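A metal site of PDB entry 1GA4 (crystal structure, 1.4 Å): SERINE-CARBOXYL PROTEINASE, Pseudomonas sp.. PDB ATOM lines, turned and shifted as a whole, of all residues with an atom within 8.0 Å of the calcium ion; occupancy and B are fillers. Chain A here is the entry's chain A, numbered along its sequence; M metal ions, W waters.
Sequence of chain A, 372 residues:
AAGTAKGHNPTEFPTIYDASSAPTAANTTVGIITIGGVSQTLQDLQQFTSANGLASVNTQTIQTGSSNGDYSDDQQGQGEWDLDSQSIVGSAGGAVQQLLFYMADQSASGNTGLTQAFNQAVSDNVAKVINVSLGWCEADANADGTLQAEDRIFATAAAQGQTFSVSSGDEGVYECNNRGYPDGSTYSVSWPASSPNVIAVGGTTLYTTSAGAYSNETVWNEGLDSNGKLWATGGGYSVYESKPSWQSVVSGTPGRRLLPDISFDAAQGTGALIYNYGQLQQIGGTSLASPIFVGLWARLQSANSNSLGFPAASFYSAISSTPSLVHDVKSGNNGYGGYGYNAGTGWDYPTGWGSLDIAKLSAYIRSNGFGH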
ATOM      1  N   VAL A 219       5.167   5.136   4.224  1.00  0.00           N
ATOM      2  CA  VAL A 219       5.922   5.365   3.000  1.00  0.00           C
ATOM      3  C   VAL A 219       7.294   5.930   3.315  1.00  0.00           C
ATOM      4  O   VAL A 219       7.436   6.785   4.197  1.00  0.00           O
ATOM      5  CB  VAL A 219       5.120   6.331   2.111  1.00  0.00           C
ATOM      6  CG1 VAL A 219       5.878   6.752   0.865  1.00  0.00           C
ATOM      7  CG2 VAL A 219       3.786   5.752   1.708  1.00  0.00           C
ATOM      8  N   VAL A 326       0.791  -9.738   3.767  1.00  0.00           N
ATOM      9  CA  VAL A 326       1.584  -8.525   3.689  1.00  0.00           C
ATOM     10  C   VAL A 326       1.319  -7.603   4.864  1.00  0.00           C
ATOM     11  O   VAL A 326       0.291  -7.682   5.540  1.00  0.00           O
ATOM     12  CB  VAL A 326       1.333  -7.737   2.382  1.00  0.00           C
ATOM     13  CG1 VAL A 326       1.838  -8.537   1.190  1.00  0.00           C
ATOM     14  CG2 VAL A 326      -0.140  -7.347   2.236  1.00  0.00           C
ATOM     15  N   HIS A 327       2.266  -6.693   5.077  1.00  0.00           N
ATOM     16  CA  HIS A 327       2.061  -5.515   5.892  1.00  0.00           C
ATOM     17  C   HIS A 327       1.640  -4.397   4.926  1.00  0.00           C
ATOM     18  O   HIS A 327       2.483  -3.939   4.151  1.00  0.00           O
ATOM     19  CB  HIS A 327       3.307  -5.073   6.631  1.00  0.00           C
ATOM     20  CG  HIS A 327       3.889  -6.113   7.563  1.00  0.00           C
ATOM     21  ND1 HIS A 327       3.231  -6.469   8.734  1.00  0.00           N
ATOM     22  CD2 HIS A 327       5.020  -6.830   7.586  1.00  0.00           C
ATOM     23  CE1 HIS A 327       3.935  -7.369   9.391  1.00  0.00           C
ATOM     24  NE2 HIS A 327       5.016  -7.614   8.714  1.00  0.00           N
ATOM     25  N   ASP A 328       0.364  -4.048   4.991  1.00  0.00           N
ATOM     26  CA  ASP A 328      -0.192  -3.059   4.086  1.00  0.00           C
ATOM     27  C   ASP A 328       0.161  -1.652   4.547  1.00  0.00           C
ATOM     28  O   ASP A 328      -0.327  -1.162   5.545  1.00  0.00           O
ATOM     29  CB  ASP A 328      -1.719  -3.216   4.042  1.00  0.00           C
ATOM     30  CG  ASP A 328      -2.424  -2.290   3.069  1.00  0.00           C
ATOM     31  OD1 ASP A 328      -1.713  -1.734   2.179  1.00  0.00           O
ATOM     32  OD2 ASP A 328      -3.642  -2.137   3.229  1.00  0.00           O
ATOM     33  N   VAL A 329       0.991  -0.924   3.822  1.00  0.00           N
ATOM     34  CA  VAL A 329       1.365   0.431   4.139  1.00  0.00           C
ATOM     35  C   VAL A 329       0.157   1.326   3.790  1.00  0.00           C
ATOM     36  O   VAL A 329      -0.386   1.199   2.692  1.00  0.00           O
ATOM     37  CB  VAL A 329       2.625   0.843   3.371  1.00  0.00           C
ATOM     38  CG1 VAL A 329       2.910   2.304   3.643  1.00  0.00           C
ATOM     39  CG2 VAL A 329       3.796  -0.043   3.767  1.00  0.00           C
ATOM     40  N   LYS A 330      -0.240   2.203   4.705  1.00  0.00           N
ATOM     41  CA  LYS A 330      -1.417   3.046   4.525  1.00  0.00           C
ATOM     42  C   LYS A 330      -1.110   4.545   4.653  1.00  0.00           C
ATOM     43  O   LYS A 330      -1.935   5.365   4.213  1.00  0.00           O
ATOM     44  CB  LYS A 330      -2.481   2.642   5.539  1.00  0.00           C
ATOM     45  CG  LYS A 330      -3.028   1.233   5.304  1.00  0.00           C
ATOM     46  CD  LYS A 330      -3.979   0.856   6.439  1.00  0.00           C
ATOM     47  CE  LYS A 330      -4.755  -0.412   6.192  1.00  0.00           C
ATOM     48  NZ  LYS A 330      -5.664  -0.651   7.342  1.00  0.00           N
ATOM     49  N   SER A 331       0.020   4.963   5.230  1.00  0.00           N
ATOM     50  CA  SER A 331       0.292   6.340   5.521  1.00  0.00           C
ATOM     51  C   SER A 331       1.518   6.885   4.777  1.00  0.00           C
ATOM     52  O   SER A 331       2.549   6.233   4.821  1.00  0.00           O
ATOM     53  CB  SER A 331       0.541   6.495   7.031  1.00  0.00           C
ATOM     54  OG  SER A 331       0.949   7.825   7.291  1.00  0.00           O
ATOM     55  N   ASN A 342      -0.460   8.931  -2.855  1.00  0.00           N
ATOM     56  CA  ASN A 342      -0.673   8.620  -1.435  1.00  0.00           C
ATOM     57  C   ASN A 342      -0.796   7.138  -1.207  1.00  0.00           C
ATOM     58  O   ASN A 342      -1.425   6.450  -2.011  1.00  0.00           O
ATOM     59  CB  ASN A 342      -1.933   9.295  -0.924  1.00  0.00           C
ATOM     60  CG  ASN A 342      -1.817  10.798  -1.054  1.00  0.00           C
ATOM     61  OD1 ASN A 342      -0.908  11.386  -0.472  1.00  0.00           O
ATOM     62  ND2 ASN A 342      -2.743  11.380  -1.801  1.00  0.00           N
ATOM     63  N   ALA A 343      -0.261   6.663  -0.090  1.00  0.00           N
ATOM     64  CA  ALA A 343      -0.560   5.290   0.282  1.00  0.00           C
ATOM     65  C   ALA A 343      -2.011   5.166   0.709  1.00  0.00           C
ATOM     66  O   ALA A 343      -2.709   6.114   1.013  1.00  0.00           O
ATOM     67  CB  ALA A 343       0.359   4.836   1.427  1.00  0.00           C
ATOM     68  N   GLY A 344      -2.493   3.912   0.720  1.00  0.00           N
ATOM     69  CA  GLY A 344      -3.866   3.676   1.112  1.00  0.00           C
ATOM     70  C   GLY A 344      -4.096   2.180   1.308  1.00  0.00           C
ATOM     71  O   GLY A 344      -3.159   1.375   1.256  1.00  0.00           O
ATOM     72  N   THR A 345      -5.346   1.804   1.539  1.00  0.00           N
ATOM     73  CA  THR A 345      -5.684   0.408   1.711  1.00  0.00           C
ATOM     74  C   THR A 345      -5.356  -0.378   0.461  1.00  0.00           C
ATOM     75  O   THR A 345      -5.698   0.027  -0.642  1.00  0.00           O
ATOM     76  CB  THR A 345      -7.181   0.300   2.014  1.00  0.00           C
ATOM     77  OG1 THR A 345      -7.422   0.981   3.248  1.00  0.00           O
ATOM     78  CG2 THR A 345      -7.612  -1.135   2.168  1.00  0.00           C
ATOM     79  N   GLY A 346      -4.686  -1.505   0.630  1.00  0.00           N
ATOM     80  CA  GLY A 346      -4.343  -2.376  -0.458  1.00  0.00           C
ATOM     81  C   GLY A 346      -3.208  -1.792  -1.330  1.00  0.00           C
ATOM     82  O   GLY A 346      -2.348  -1.050  -0.848  1.00  0.00           O
ATOM     83  N   TRP A 347      -3.170  -2.185  -2.583  1.00  0.00           N
ATOM     84  CA  TRP A 347      -2.073  -1.791  -3.464  1.00  0.00           C
ATOM     85  C   TRP A 347      -2.104  -0.289  -3.628  1.00  0.00           C
ATOM     86  O   TRP A 347      -3.182   0.269  -3.864  1.00  0.00           O
ATOM     87  CB  TRP A 347      -2.213  -2.524  -4.803  1.00  0.00           C
ATOM     88  CG  TRP A 347      -0.993  -2.349  -5.676  1.00  0.00           C
ATOM     89  CD1 TRP A 347       0.002  -3.297  -5.841  1.00  0.00           C
ATOM     90  CD2 TRP A 347      -0.608  -1.238  -6.488  1.00  0.00           C
ATOM     91  NE1 TRP A 347       0.936  -2.824  -6.685  1.00  0.00           N
ATOM     92  CE2 TRP A 347       0.601  -1.555  -7.093  1.00  0.00           C
ATOM     93  CE3 TRP A 347      -1.165   0.011  -6.779  1.00  0.00           C
ATOM     94  CZ2 TRP A 347       1.259  -0.694  -7.949  1.00  0.00           C
ATOM     95  CZ3 TRP A 347      -0.522   0.901  -7.619  1.00  0.00           C
ATOM     96  CH2 TRP A 347       0.688   0.520  -8.196  1.00  0.00           C
ATOM     97  N   ASP A 348      -0.968   0.374  -3.542  1.00  0.00           N
ATOM     98  CA  ASP A 348      -0.892   1.814  -3.827  1.00  0.00           C
ATOM     99  C   ASP A 348       0.396   2.104  -4.601  1.00  0.00           C
ATOM    100  O   ASP A 348       1.311   1.296  -4.683  1.00  0.00           O
ATOM    101  CB  ASP A 348      -1.037   2.575  -2.530  1.00  0.00           C
ATOM    102  CG  ASP A 348      -0.011   2.236  -1.445  1.00  0.00           C
ATOM    103  OD1 ASP A 348       1.217   2.344  -1.726  1.00  0.00           O
ATOM    104  OD2 ASP A 348      -0.506   1.909  -0.343  1.00  0.00           O
ATOM    105  N   TYR A 349       0.425   3.333  -5.185  1.00  0.00           N
ATOM    106  CA  TYR A 349       1.566   3.644  -6.005  1.00  0.00           C
ATOM    107  C   TYR A 349       2.872   3.861  -5.229  1.00  0.00           C
ATOM    108  O   TYR A 349       3.950   3.563  -5.779  1.00  0.00           O
ATOM    109  CB  TYR A 349       1.253   4.867  -6.850  1.00  0.00           C
ATOM    110  CG  TYR A 349       0.306   4.605  -7.994  1.00  0.00           C
ATOM    111  CD1 TYR A 349      -1.006   5.065  -7.972  1.00  0.00           C
ATOM    112  CD2 TYR A 349       0.773   3.865  -9.094  1.00  0.00           C
ATOM    113  CE1 TYR A 349      -1.833   4.793  -9.062  1.00  0.00           C
ATOM    114  CE2 TYR A 349      -0.051   3.608 -10.164  1.00  0.00           C
ATOM    115  CZ  TYR A 349      -1.363   4.068 -10.143  1.00  0.00           C
ATOM    116  OH  TYR A 349      -2.176   3.791 -11.241  1.00  0.00           O
ATOM    117  N   PRO A 350       2.914   4.403  -4.011  1.00  0.00           N
ATOM    118  CA  PRO A 350       4.211   4.478  -3.339  1.00  0.00           C
ATOM    119  C   PRO A 350       4.861   3.137  -2.985  1.00  0.00           C
ATOM    120  O   PRO A 350       6.081   3.008  -3.057  1.00  0.00           O
ATOM    121  CB  PRO A 350       3.914   5.292  -2.082  1.00  0.00           C
ATOM    122  CG  PRO A 350       2.730   6.156  -2.507  1.00  0.00           C
ATOM    123  CD  PRO A 350       1.875   5.184  -3.294  1.00  0.00           C
ATOM    124  N   THR A 351       4.038   2.155  -2.582  1.00  0.00           N
ATOM    125  CA  THR A 351       4.532   0.940  -1.955  1.00  0.00           C
ATOM    126  C   THR A 351       4.042  -0.382  -2.531  1.00  0.00           C
ATOM    127  O   THR A 351       4.449  -1.457  -2.043  1.00  0.00           O
ATOM    128  CB  THR A 351       4.258   0.953  -0.423  1.00  0.00           C
ATOM    129  OG1 THR A 351       2.863   1.000  -0.115  1.00  0.00           O
ATOM    130  CG2 THR A 351       4.958   2.131   0.215  1.00  0.00           C
ATOM    131  N   GLY A 352       3.160  -0.342  -3.517  1.00  0.00           N
ATOM    132  CA  GLY A 352       2.584  -1.537  -4.079  1.00  0.00           C
ATOM    133  C   GLY A 352       1.812  -2.292  -3.006  1.00  0.00           C
ATOM    134  O   GLY A 352       1.030  -1.640  -2.298  1.00  0.00           O
ATOM    135  N   TRP A 353       2.025  -3.603  -2.869  1.00  0.00           N
ATOM    136  CA  TRP A 353       1.295  -4.354  -1.836  1.00  0.00           C
ATOM    137  C   TRP A 353       1.873  -4.147  -0.444  1.00  0.00           C
ATOM    138  O   TRP A 353       1.281  -4.667   0.516  1.00  0.00           O
ATOM    139  CB  TRP A 353       1.360  -5.825  -2.188  1.00  0.00           C
ATOM    140  CG  TRP A 353       0.582  -6.223  -3.392  1.00  0.00           C
ATOM    141  CD1 TRP A 353       1.075  -6.710  -4.561  1.00  0.00           C
ATOM    142  CD2 TRP A 353      -0.837  -6.179  -3.537  1.00  0.00           C
ATOM    143  NE1 TRP A 353       0.054  -6.961  -5.416  1.00  0.00           N
ATOM    144  CE2 TRP A 353      -1.142  -6.650  -4.820  1.00  0.00           C
ATOM    145  CE3 TRP A 353      -1.896  -5.791  -2.715  1.00  0.00           C
ATOM    146  CZ2 TRP A 353      -2.458  -6.742  -5.289  1.00  0.00           C
ATOM    147  CZ3 TRP A 353      -3.185  -5.891  -3.172  1.00  0.00           C
ATOM    148  CH2 TRP A 353      -3.481  -6.358  -4.466  1.00  0.00           C
ATOM    149  N   GLY A 354       2.993  -3.492  -0.267  1.00  0.00           N
ATOM    150  CA  GLY A 354       3.674  -3.428   1.013  1.00  0.00           C
ATOM    151  C   GLY A 354       4.711  -4.505   1.166  1.00  0.00           C
ATOM    152  O   GLY A 354       5.191  -5.044   0.174  1.00  0.00           O
HETATM  153 CA    CA M   1      -1.256   0.107   0.861  1.00  0.00          CA
HETATM  154  O   HOH W   1       0.876  -0.889   0.350  1.00  0.00           O
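Water W1 lies within hydrogen-bond range of the backbone carbonyl oxygen of Gly 352, the side-chain hydroxyl of Thr 351, the backbone NH of Gly 354 and the backbone NH of Val 329.
The calcium ion is bound by OD2 of Asp 348 (2.3 Å), O of Val 329 (2.3 Å), OD1 of Asp 328 (2.3 Å), O of Gly 344 (2.3 Å), O of Gly 346 (2.3 Å) and water W1 (2.4 Å).
The side-chain hydroxyl (OG1) of Thr 351 lies within hydrogen-bond range of the side-chain carboxylate (OD1) of Asp 348, at 2.7 Å.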
